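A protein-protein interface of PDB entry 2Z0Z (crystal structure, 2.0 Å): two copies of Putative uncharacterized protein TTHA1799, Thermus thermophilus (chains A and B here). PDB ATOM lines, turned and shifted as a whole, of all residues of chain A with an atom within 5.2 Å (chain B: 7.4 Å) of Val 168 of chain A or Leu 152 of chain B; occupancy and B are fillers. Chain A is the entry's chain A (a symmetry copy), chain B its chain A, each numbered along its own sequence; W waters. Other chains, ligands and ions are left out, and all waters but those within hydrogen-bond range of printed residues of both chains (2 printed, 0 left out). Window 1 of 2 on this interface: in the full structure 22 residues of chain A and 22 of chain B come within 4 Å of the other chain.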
ATOM      1  N   ARG A 125      13.170 -15.729  -7.143  1.00  0.00           N
ATOM      2  CA  ARG A 125      12.038 -15.472  -6.263  1.00  0.00           C
ATOM      3  C   ARG A 125      12.274 -15.873  -4.822  1.00  0.00           C
ATOM      4  O   ARG A 125      12.728 -16.994  -4.552  1.00  0.00           O
ATOM      5  CB  ARG A 125      10.797 -16.257  -6.771  1.00  0.00           C
ATOM      6  CG  ARG A 125       9.586 -16.283  -5.780  1.00  0.00           C
ATOM      7  CD  ARG A 125       8.450 -17.302  -6.193  1.00  0.00           C
ATOM      8  NE  ARG A 125       7.338 -17.324  -5.220  1.00  0.00           N
ATOM      9  CZ  ARG A 125       6.344 -16.438  -5.188  1.00  0.00           C
ATOM     10  NH1 ARG A 125       6.288 -15.453  -6.087  1.00  0.00           N
ATOM     11  NH2 ARG A 125       5.428 -16.499  -4.225  1.00  0.00           N
ATOM     12  N   GLN A 127       9.989 -15.959  -1.415  1.00  0.00           N
ATOM     13  CA  GLN A 127       8.646 -15.821  -0.893  1.00  0.00           C
ATOM     14  C   GLN A 127       8.637 -15.708   0.633  1.00  0.00           C
ATOM     15  O   GLN A 127       9.558 -16.193   1.322  1.00  0.00           O
ATOM     16  CB  GLN A 127       7.847 -17.049  -1.337  1.00  0.00           C
ATOM     17  CG  GLN A 127       6.604 -17.407  -0.536  1.00  0.00           C
ATOM     18  CD  GLN A 127       5.927 -18.625  -1.155  1.00  0.00           C
ATOM     19  OE1 GLN A 127       5.536 -18.588  -2.328  1.00  0.00           O
ATOM     20  NE2 GLN A 127       5.809 -19.710  -0.385  1.00  0.00           N
ATOM     21  N   PHE A 128       7.607 -15.037   1.137  1.00  0.00           N
ATOM     22  CA  PHE A 128       7.360 -14.898   2.566  1.00  0.00           C
ATOM     23  C   PHE A 128       5.913 -15.346   2.727  1.00  0.00           C
ATOM     24  O   PHE A 128       5.060 -15.029   1.883  1.00  0.00           O
ATOM     25  CB  PHE A 128       7.482 -13.441   3.008  1.00  0.00           C
ATOM     26  CG  PHE A 128       8.851 -12.880   2.854  1.00  0.00           C
ATOM     27  CD1 PHE A 128       9.807 -13.078   3.841  1.00  0.00           C
ATOM     28  CD2 PHE A 128       9.195 -12.165   1.710  1.00  0.00           C
ATOM     29  CE1 PHE A 128      11.103 -12.563   3.698  1.00  0.00           C
ATOM     30  CE2 PHE A 128      10.487 -11.646   1.554  1.00  0.00           C
ATOM     31  CZ  PHE A 128      11.440 -11.849   2.558  1.00  0.00           C
ATOM     32  N   LYS A 129       5.623 -16.086   3.791  1.00  0.00           N
ATOM     33  CA  LYS A 129       4.262 -16.535   4.013  1.00  0.00           C
ATOM     34  C   LYS A 129       3.936 -16.320   5.483  1.00  0.00           C
ATOM     35  O   LYS A 129       4.662 -16.790   6.367  1.00  0.00           O
ATOM     36  CB  LYS A 129       4.126 -18.007   3.602  1.00  0.00           C
ATOM     37  CG  LYS A 129       2.734 -18.564   3.670  1.00  0.00           C
ATOM     38  CD  LYS A 129       2.541 -19.700   2.655  1.00  0.00           C
ATOM     39  CE  LYS A 129       3.478 -20.867   2.884  1.00  0.00           C
ATOM     40  NZ  LYS A 129       3.264 -21.482   4.221  1.00  0.00           N
ATOM     41  N   VAL A 147       5.986  -7.720  -2.330  1.00  0.00           N
ATOM     42  CA  VAL A 147       4.712  -7.586  -2.998  1.00  0.00           C
ATOM     43  C   VAL A 147       3.696  -8.575  -2.444  1.00  0.00           C
ATOM     44  O   VAL A 147       3.976  -9.775  -2.360  1.00  0.00           O
ATOM     45  CB  VAL A 147       4.885  -7.814  -4.520  1.00  0.00           C
ATOM     46  CG1 VAL A 147       3.541  -7.881  -5.199  1.00  0.00           C
ATOM     47  CG2 VAL A 147       5.746  -6.683  -5.118  1.00  0.00           C
ATOM     48  N   ARG A 148       2.523  -8.077  -2.058  1.00  0.00           N
ATOM     49  CA  ARG A 148       1.465  -8.947  -1.515  1.00  0.00           C
ATOM     50  C   ARG A 148       0.800  -9.639  -2.716  1.00  0.00           C
ATOM     51  O   ARG A 148       0.092  -8.993  -3.498  1.00  0.00           O
ATOM     52  CB  ARG A 148       0.426  -8.115  -0.757  1.00  0.00           C
ATOM     53  CG  ARG A 148      -0.557  -8.925   0.099  1.00  0.00           C
ATOM     54  CD  ARG A 148      -1.639  -8.005   0.688  1.00  0.00           C
ATOM     55  NE  ARG A 148      -2.701  -8.732   1.379  1.00  0.00           N
ATOM     56  CZ  ARG A 148      -2.800  -8.851   2.703  1.00  0.00           C
ATOM     57  NH1 ARG A 148      -1.901  -8.286   3.504  1.00  0.00           N
ATOM     58  NH2 ARG A 148      -3.797  -9.549   3.230  1.00  0.00           N
ATOM     59  N   GLU A 149       1.023 -10.941  -2.877  1.00  0.00           N
ATOM     60  CA  GLU A 149       0.440 -11.640  -4.022  1.00  0.00           C
ATOM     61  C   GLU A 149      -0.996 -12.126  -3.787  1.00  0.00           C
ATOM     62  O   GLU A 149      -1.807 -12.174  -4.720  1.00  0.00           O
ATOM     63  CB  GLU A 149       1.359 -12.803  -4.450  1.00  0.00           C
ATOM     64  CG  GLU A 149       2.738 -12.310  -4.913  1.00  0.00           C
ATOM     65  CD  GLU A 149       3.671 -13.431  -5.364  1.00  0.00           C
ATOM     66  OE1 GLU A 149       3.575 -14.533  -4.799  1.00  0.00           O
ATOM     67  OE2 GLU A 149       4.511 -13.196  -6.267  1.00  0.00           O
ATOM     68  N   GLY A 150      -1.323 -12.482  -2.552  1.00  0.00           N
ATOM     69  CA  GLY A 150      -2.673 -12.952  -2.296  1.00  0.00           C
ATOM     70  C   GLY A 150      -2.807 -13.737  -1.009  1.00  0.00           C
ATOM     71  O   GLY A 150      -1.822 -13.910  -0.274  1.00  0.00           O
ATOM     72  N   VAL A 151      -4.020 -14.216  -0.734  1.00  0.00           N
ATOM     73  CA  VAL A 151      -4.277 -14.970   0.483  1.00  0.00           C
ATOM     74  C   VAL A 151      -4.699 -16.400   0.164  1.00  0.00           C
ATOM     75  O   VAL A 151      -5.676 -16.626  -0.563  1.00  0.00           O
ATOM     76  CB  VAL A 151      -5.382 -14.292   1.327  1.00  0.00           C
ATOM     77  CG1 VAL A 151      -5.752 -15.158   2.542  1.00  0.00           C
ATOM     78  CG2 VAL A 151      -4.907 -12.924   1.789  1.00  0.00           C
ATOM     79  N   LEU A 152      -3.940 -17.358   0.680  1.00  0.00           N
ATOM     80  CA  LEU A 152      -4.254 -18.768   0.469  1.00  0.00           C
ATOM     81  C   LEU A 152      -5.213 -19.060   1.614  1.00  0.00           C
ATOM     82  O   LEU A 152      -4.793 -19.178   2.764  1.00  0.00           O
ATOM     83  CB  LEU A 152      -2.986 -19.622   0.572  1.00  0.00           C
ATOM     84  CG  LEU A 152      -1.890 -19.254  -0.440  1.00  0.00           C
ATOM     85  CD1 LEU A 152      -0.602 -20.087  -0.185  1.00  0.00           C
ATOM     86  CD2 LEU A 152      -2.412 -19.500  -1.867  1.00  0.00           C
ATOM     87  N   ASP A 166      -3.110 -17.942   4.961  1.00  0.00           N
ATOM     88  CA  ASP A 166      -1.732 -17.507   4.755  1.00  0.00           C
ATOM     89  C   ASP A 166      -1.670 -16.405   3.720  1.00  0.00           C
ATOM     90  O   ASP A 166      -2.256 -16.535   2.643  1.00  0.00           O
ATOM     91  CB  ASP A 166      -0.844 -18.644   4.234  1.00  0.00           C
ATOM     92  CG  ASP A 166      -0.412 -19.599   5.325  1.00  0.00           C
ATOM     93  OD1 ASP A 166      -0.217 -19.129   6.463  1.00  0.00           O
ATOM     94  OD2 ASP A 166      -0.247 -20.806   5.019  1.00  0.00           O
ATOM     95  N   VAL A 167      -0.949 -15.331   4.029  1.00  0.00           N
ATOM     96  CA  VAL A 167      -0.780 -14.252   3.077  1.00  0.00           C
ATOM     97  C   VAL A 167       0.580 -14.513   2.425  1.00  0.00           C
ATOM     98  O   VAL A 167       1.569 -14.730   3.127  1.00  0.00           O
ATOM     99  CB  VAL A 167      -0.721 -12.875   3.774  1.00  0.00           C
ATOM    100  CG1 VAL A 167      -0.635 -11.779   2.730  1.00  0.00           C
ATOM    101  CG2 VAL A 167      -1.939 -12.691   4.684  1.00  0.00           C
ATOM    102  N   VAL A 168       0.633 -14.497   1.098  1.00  0.00           N
ATOM    103  CA  VAL A 168       1.885 -14.737   0.397  1.00  0.00           C
ATOM    104  C   VAL A 168       2.451 -13.440  -0.149  1.00  0.00           C
ATOM    105  O   VAL A 168       1.736 -12.664  -0.790  1.00  0.00           O
ATOM    106  CB  VAL A 168       1.704 -15.730  -0.788  1.00  0.00           C
ATOM    107  CG1 VAL A 168       3.054 -15.978  -1.488  1.00  0.00           C
ATOM    108  CG2 VAL A 168       1.145 -17.037  -0.283  1.00  0.00           C
ATOM    109  N   TYR A 169       3.741 -13.226   0.105  1.00  0.00           N
ATOM    110  CA  TYR A 169       4.464 -12.041  -0.373  1.00  0.00           C
ATOM    111  C   TYR A 169       5.681 -12.542  -1.108  1.00  0.00           C
ATOM    112  O   TYR A 169       6.133 -13.659  -0.860  1.00  0.00           O
ATOM    113  CB  TYR A 169       4.987 -11.195   0.791  1.00  0.00           C
ATOM    114  CG  TYR A 169       3.958 -10.417   1.547  1.00  0.00           C
ATOM    115  CD1 TYR A 169       3.695  -9.079   1.233  1.00  0.00           C
ATOM    116  CD2 TYR A 169       3.254 -11.006   2.595  1.00  0.00           C
ATOM    117  CE1 TYR A 169       2.751  -8.339   1.961  1.00  0.00           C
ATOM    118  CE2 TYR A 169       2.315 -10.280   3.318  1.00  0.00           C
ATOM    119  CZ  TYR A 169       2.076  -8.954   2.997  1.00  0.00           C
ATOM    120  OH  TYR A 169       1.178  -8.247   3.747  1.00  0.00           O
ATOM    121  N   SER A 170       6.220 -11.724  -2.006  1.00  0.00           N
ATOM    122  CA  SER A 170       7.451 -12.118  -2.667  1.00  0.00           C
ATOM    123  C   SER A 170       8.270 -10.921  -3.085  1.00  0.00           C
ATOM    124  O   SER A 170       7.752  -9.799  -3.218  1.00  0.00           O
ATOM    125  CB  SER A 170       7.185 -12.984  -3.905  1.00  0.00           C
ATOM    126  OG  SER A 170       6.688 -12.212  -4.985  1.00  0.00           O
ATOM    127  N   GLN B 127      -7.106 -26.796  -4.044  1.00  0.00           N
ATOM    128  CA  GLN B 127      -6.467 -25.761  -4.828  1.00  0.00           C
ATOM    129  C   GLN B 127      -6.269 -26.189  -6.283  1.00  0.00           C
ATOM    130  O   GLN B 127      -6.177 -27.394  -6.595  1.00  0.00           O
ATOM    131  CB  GLN B 127      -5.115 -25.455  -4.178  1.00  0.00           C
ATOM    132  CG  GLN B 127      -4.050 -24.801  -5.045  1.00  0.00           C
ATOM    133  CD  GLN B 127      -2.799 -24.539  -4.212  1.00  0.00           C
ATOM    134  OE1 GLN B 127      -2.862 -23.820  -3.208  1.00  0.00           O
ATOM    135  NE2 GLN B 127      -1.672 -25.137  -4.607  1.00  0.00           N
ATOM    136  N   LYS B 129      -3.872 -24.782  -9.671  1.00  0.00           N
ATOM    137  CA  LYS B 129      -2.782 -23.882  -9.994  1.00  0.00           C
ATOM    138  C   LYS B 129      -2.526 -23.979 -11.490  1.00  0.00           C
ATOM    139  O   LYS B 129      -2.314 -25.074 -12.025  1.00  0.00           O
ATOM    140  CB  LYS B 129      -1.540 -24.252  -9.172  1.00  0.00           C
ATOM    141  CG  LYS B 129      -0.371 -23.323  -9.322  1.00  0.00           C
ATOM    142  CD  LYS B 129       0.497 -23.314  -8.056  1.00  0.00           C
ATOM    143  CE  LYS B 129       1.074 -24.673  -7.722  1.00  0.00           C
ATOM    144  NZ  LYS B 129       1.956 -25.172  -8.811  1.00  0.00           N
ATOM    145  N   VAL B 130      -2.588 -22.839 -12.169  1.00  0.00           N
ATOM    146  CA  VAL B 130      -2.392 -22.822 -13.613  1.00  0.00           C
ATOM    147  C   VAL B 130      -1.502 -21.679 -14.094  1.00  0.00           C
ATOM    148  O   VAL B 130      -1.375 -20.650 -13.441  1.00  0.00           O
ATOM    149  CB  VAL B 130      -3.752 -22.771 -14.355  1.00  0.00           C
ATOM    150  CG1 VAL B 130      -4.554 -24.064 -14.080  1.00  0.00           C
ATOM    151  CG2 VAL B 130      -4.555 -21.558 -13.905  1.00  0.00           C
ATOM    152  N   LEU B 132      -0.228 -18.452 -15.826  1.00  0.00           N
ATOM    153  CA  LEU B 132      -0.924 -17.204 -16.102  1.00  0.00           C
ATOM    154  C   LEU B 132      -1.218 -17.078 -17.608  1.00  0.00           C
ATOM    155  O   LEU B 132      -2.142 -16.376 -18.000  1.00  0.00           O
ATOM    156  CB  LEU B 132      -0.080 -16.006 -15.642  1.00  0.00           C
ATOM    157  CG  LEU B 132      -0.689 -14.601 -15.823  1.00  0.00           C
ATOM    158  CD1 LEU B 132      -1.946 -14.455 -14.949  1.00  0.00           C
ATOM    159  CD2 LEU B 132       0.357 -13.537 -15.443  1.00  0.00           C
ATOM    160  N   GLY B 150      -4.741 -15.353  -6.233  1.00  0.00           N
ATOM    161  CA  GLY B 150      -3.632 -14.482  -6.579  1.00  0.00           C
ATOM    162  C   GLY B 150      -2.654 -15.104  -7.552  1.00  0.00           C
ATOM    163  O   GLY B 150      -2.849 -16.248  -7.994  1.00  0.00           O
ATOM    164  N   VAL B 151      -1.599 -14.360  -7.887  1.00  0.00           N
ATOM    165  CA  VAL B 151      -0.601 -14.842  -8.828  1.00  0.00           C
ATOM    166  C   VAL B 151       0.761 -14.981  -8.159  1.00  0.00           C
ATOM    167  O   VAL B 151       1.295 -14.015  -7.597  1.00  0.00           O
ATOM    168  CB  VAL B 151      -0.477 -13.884 -10.036  1.00  0.00           C
ATOM    169  CG1 VAL B 151       0.672 -14.317 -10.962  1.00  0.00           C
ATOM    170  CG2 VAL B 151      -1.787 -13.861 -10.808  1.00  0.00           C
ATOM    171  N   LEU B 152       1.303 -16.192  -8.191  1.00  0.00           N
ATOM    172  CA  LEU B 152       2.617 -16.449  -7.609  1.00  0.00           C
ATOM    173  C   LEU B 152       3.552 -16.118  -8.762  1.00  0.00           C
ATOM    174  O   LEU B 152       3.665 -16.888  -9.714  1.00  0.00           O
ATOM    175  CB  LEU B 152       2.742 -17.919  -7.194  1.00  0.00           C
ATOM    176  CG  LEU B 152       1.701 -18.377  -6.162  1.00  0.00           C
ATOM    177  CD1 LEU B 152       1.826 -19.903  -5.891  1.00  0.00           C
ATOM    178  CD2 LEU B 152       1.894 -17.584  -4.856  1.00  0.00           C
ATOM    179  N   ARG B 153       4.192 -14.953  -8.691  1.00  0.00           N
ATOM    180  CA  ARG B 153       5.072 -14.502  -9.773  1.00  0.00           C
ATOM    181  C   ARG B 153       6.378 -15.309  -9.878  1.00  0.00           C
ATOM    182  O   ARG B 153       7.053 -15.540  -8.877  1.00  0.00           O
ATOM    183  CB  ARG B 153       5.390 -13.013  -9.581  1.00  0.00           C
ATOM    184  CG  ARG B 153       4.135 -12.131  -9.403  1.00  0.00           C
ATOM    185  CD  ARG B 153       4.507 -10.693  -9.008  1.00  0.00           C
ATOM    186  NE  ARG B 153       5.338 -10.669  -7.797  1.00  0.00           N
ATOM    187  CZ  ARG B 153       6.171  -9.678  -7.500  1.00  0.00           C
ATOM    188  NH1 ARG B 153       6.260  -8.641  -8.327  1.00  0.00           N
ATOM    189  NH2 ARG B 153       6.946  -9.738  -6.413  1.00  0.00           N
ATOM    190  N   LYS B 154       6.731 -15.710 -11.098  1.00  0.00           N
ATOM    191  CA  LYS B 154       7.955 -16.479 -11.349  1.00  0.00           C
ATOM    192  C   LYS B 154       8.000 -17.688 -10.421  1.00  0.00           C
ATOM    193  O   LYS B 154       9.039 -17.975  -9.815  1.00  0.00           O
ATOM    194  CB  LYS B 154       9.200 -15.637 -11.065  1.00  0.00           C
ATOM    195  CG  LYS B 154       9.174 -14.222 -11.586  1.00  0.00           C
ATOM    196  CD  LYS B 154       9.156 -14.180 -13.078  1.00  0.00           C
ATOM    197  CE  LYS B 154       9.391 -12.751 -13.574  1.00  0.00           C
ATOM    198  NZ  LYS B 154       9.096 -12.643 -15.038  1.00  0.00           N
ATOM    199  N   ASN B 155       6.883 -18.394 -10.330  1.00  0.00           N
ATOM    200  CA  ASN B 155       6.772 -19.539  -9.445  1.00  0.00           C
ATOM    201  C   ASN B 155       7.369 -20.837  -9.965  1.00  0.00           C
ATOM    202  O   ASN B 155       7.536 -21.783  -9.200  1.00  0.00           O
ATOM    203  CB  ASN B 155       5.313 -19.742  -9.054  1.00  0.00           C
ATOM    204  CG  ASN B 155       5.174 -20.605  -7.825  1.00  0.00           C
ATOM    205  OD1 ASN B 155       5.818 -20.350  -6.804  1.00  0.00           O
ATOM    206  ND2 ASN B 155       4.342 -21.632  -7.912  1.00  0.00           N
ATOM    207  N   ARG B 156       7.692 -20.901 -11.256  1.00  0.00           N
ATOM    208  CA  ARG B 156       8.311 -22.101 -11.795  1.00  0.00           C
ATOM    209  C   ARG B 156       9.246 -21.707 -12.908  1.00  0.00           C
ATOM    210  O   ARG B 156       9.081 -20.650 -13.517  1.00  0.00           O
ATOM    211  CB  ARG B 156       7.268 -23.099 -12.331  1.00  0.00           C
ATOM    212  CG  ARG B 156       6.562 -22.688 -13.625  1.00  0.00           C
ATOM    213  CD  ARG B 156       5.475 -23.721 -14.016  1.00  0.00           C
ATOM    214  NE  ARG B 156       4.764 -23.388 -15.253  1.00  0.00           N
ATOM    215  CZ  ARG B 156       4.901 -24.054 -16.401  1.00  0.00           C
ATOM    216  NH1 ARG B 156       5.735 -25.090 -16.472  1.00  0.00           N
ATOM    217  NH2 ARG B 156       4.182 -23.713 -17.473  1.00  0.00           N
ATOM    218  N   ARG B 164       7.757 -18.676 -15.401  1.00  0.00           N
ATOM    219  CA  ARG B 164       6.330 -18.517 -15.643  1.00  0.00           C
ATOM    220  C   ARG B 164       5.623 -18.219 -14.317  1.00  0.00           C
ATOM    221  O   ARG B 164       6.122 -18.581 -13.250  1.00  0.00           O
ATOM    222  CB  ARG B 164       5.749 -19.773 -16.288  1.00  0.00           C
ATOM    223  CG  ARG B 164       6.251 -20.012 -17.737  1.00  0.00           C
ATOM    224  CD  ARG B 164       5.870 -18.877 -18.700  1.00  0.00           C
ATOM    225  NE  ARG B 164       6.356 -19.134 -20.063  1.00  0.00           N
ATOM    226  CZ  ARG B 164       7.447 -18.581 -20.606  1.00  0.00           C
ATOM    227  NH1 ARG B 164       8.185 -17.708 -19.917  1.00  0.00           N
ATOM    228  NH2 ARG B 164       7.828 -18.934 -21.837  1.00  0.00           N
ATOM    229  N   ASP B 165       4.476 -17.543 -14.399  1.00  0.00           N
ATOM    230  CA  ASP B 165       3.693 -17.178 -13.234  1.00  0.00           C
ATOM    231  C   ASP B 165       2.543 -18.182 -13.079  1.00  0.00           C
ATOM    232  O   ASP B 165       1.981 -18.648 -14.074  1.00  0.00           O
ATOM    233  CB  ASP B 165       3.093 -15.774 -13.395  1.00  0.00           C
ATOM    234  CG  ASP B 165       4.149 -14.681 -13.598  1.00  0.00           C
ATOM    235  OD1 ASP B 165       5.337 -14.890 -13.295  1.00  0.00           O
ATOM    236  OD2 ASP B 165       3.763 -13.587 -14.045  1.00  0.00           O
ATOM    237  N   ASP B 166       2.207 -18.498 -11.828  1.00  0.00           N
ATOM    238  CA  ASP B 166       1.122 -19.423 -11.513  1.00  0.00           C
ATOM    239  C   ASP B 166      -0.043 -18.686 -10.887  1.00  0.00           C
ATOM    240  O   ASP B 166       0.151 -17.902  -9.957  1.00  0.00           O
ATOM    241  CB  ASP B 166       1.556 -20.490 -10.501  1.00  0.00           C
ATOM    242  CG  ASP B 166       2.364 -21.604 -11.130  1.00  0.00           C
ATOM    243  OD1 ASP B 166       2.085 -21.932 -12.299  1.00  0.00           O
ATOM    244  OD2 ASP B 166       3.252 -22.153 -10.432  1.00  0.00           O
ATOM    245  N   VAL B 167      -1.251 -18.948 -11.378  1.00  0.00           N
ATOM    246  CA  VAL B 167      -2.432 -18.338 -10.802  1.00  0.00           C
ATOM    247  C   VAL B 167      -3.000 -19.398  -9.855  1.00  0.00           C
ATOM    248  O   VAL B 167      -3.167 -20.553 -10.252  1.00  0.00           O
ATOM    249  CB  VAL B 167      -3.501 -18.031 -11.875  1.00  0.00           C
ATOM    250  CG1 VAL B 167      -4.674 -17.314 -11.235  1.00  0.00           C
ATOM    251  CG2 VAL B 167      -2.888 -17.205 -13.010  1.00  0.00           C
ATOM    252  N   VAL B 168      -3.292 -19.017  -8.617  1.00  0.00           N
ATOM    253  CA  VAL B 168      -3.834 -19.961  -7.652  1.00  0.00           C
ATOM    254  C   VAL B 168      -5.318 -19.726  -7.448  1.00  0.00           C
ATOM    255  O   VAL B 168      -5.750 -18.589  -7.233  1.00  0.00           O
ATOM    256  CB  VAL B 168      -3.125 -19.848  -6.272  1.00  0.00           C
ATOM    257  CG1 VAL B 168      -3.707 -20.880  -5.285  1.00  0.00           C
ATOM    258  CG2 VAL B 168      -1.643 -20.080  -6.433  1.00  0.00           C
HETATM  259  O   HOH W   1      -1.695 -11.504  -7.194  1.00  0.00           O
HETATM  260  O   HOH W   2       5.241 -20.785  -4.116  1.00  0.00           O
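The guanidinium group of Arg 153 of chain B is in salt-bridge range of the side-chain carboxylate of Glu 149 of chain A, at 3.1 Å.
The backbone carbonyl oxygen (O) of Arg 153 of chain B is in hydrogen-bond range of the guanidinium group (NH1) of Arg 125 of chain A (2.9 Å).
NH2 of Arg 153 of chain B is in hydrogen-bond range of OG of Ser 170 of chain A (2.9 Å).
The backbone NH (N) of Leu 152 of chain B lies within hydrogen-bond range of the backbone carbonyl oxygen (O) of Asp 166 of chain B.
The backbone carbonyl oxygen (O) of Arg 164 of chain B sits at hydrogen-bond distance from the backbone NH (N) of Asn 155 of chain B.
The backbone NH of Leu 152 of chain A is in hydrogen-bond range of the backbone carbonyl oxygen of Asp 166 of chain A (2.7 Å).
O of Gly 150 of chain A sits at hydrogen-bond distance from N of Val 168 of chain A (2.9 Å).
The side-chain hydroxyl (OG) of Ser 170 of chain A sits close to the guanidinium group (NH1) of Arg 125 of chain A.
The backbone carbonyl oxygen (O) of Ser 170 of chain A sits at hydrogen-bond distance from the backbone NH (N) of Val 147 of chain A (2.9 Å).
NH2 of Arg 125 of chain A touches CD2 of Leu 152 of chain B (3.8 Å).
O of Lys 154 of chain B touches CD of Arg 125 of chain A, 3.7 Å away.
Arg 125 of chain A touches Asn 155 of chain B.
CB of Val 147 of chain A touches NH2 of Arg 153 of chain B (3.4 Å).
CA of Gly 150 of chain B touches O of Glu 149 of chain A, at 3.5 Å.
Glu 149 of chain A touches Val 151 of chain B.
OE1 of Glu 149 of chain A touches CD2 of Leu 152 of chain B, at 3.5 Å.
Leu 152 of chain A touches Val 168 of chain B (CD2 to CG1, 3.9 Å).
CG1 of Val 168 of chain A touches CD2 of Leu 152 of chain B, at 3.9 Å.
Val 168 of chain A touches just one residue of chain B: Leu 152.
Leu 152 of chain B touches just these residues of chain A: Arg 125, Glu 149 and Val 168.
Of the printed residues of chain A, Asn 155 of chain B touches Arg 125.
Of the printed residues of chain B, Val 147 of chain A touches Arg 153 (3.4 Å).
Of the printed residues of chain A, Gly 150 of chain B touches Glu 149 (3.5 Å).
Val 130 of chain B touches none of the printed residues of chain A.
The nearest residue of chain A that does not touch Leu 152 of chain B is Gln 127 of chain A (4.5 Å).
Printed residues of chain A that touch a printed residue of chain B: Arg 125, Val 147, Glu 149, Leu 152, Val 168 and Ser 170.
Among the printed residues, 12 pairs touch across the chains.
Among the printed residues, Asp or Glu carboxylates within 4 Å of a Lys or Arg side-chain nitrogen of the other chain: Glu 149 of chain A with Arg 153 of chain B (3.1 Å).
Leu 152 of chain A touches Val 168 of chain B, and with the chains exchanged Val 168 of chain A touches Leu 152 of chain B.
Of the 12 pairs that touch across the chains among the printed residues, 2 have their exchanged pair printed and touching as well.
Water W1 lies within hydrogen-bond range of the backbone carbonyl oxygen of Glu 149 of chain A (2.6 Å) and the backbone NH of Val 151 of chain B (2.9 Å).
Water W2 lies within hydrogen-bond range of the side-chain amide oxygen (OD1) of Asn 155 of chain B and the side-chain amide oxygen (OE1) of Gln 127 of chain A.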
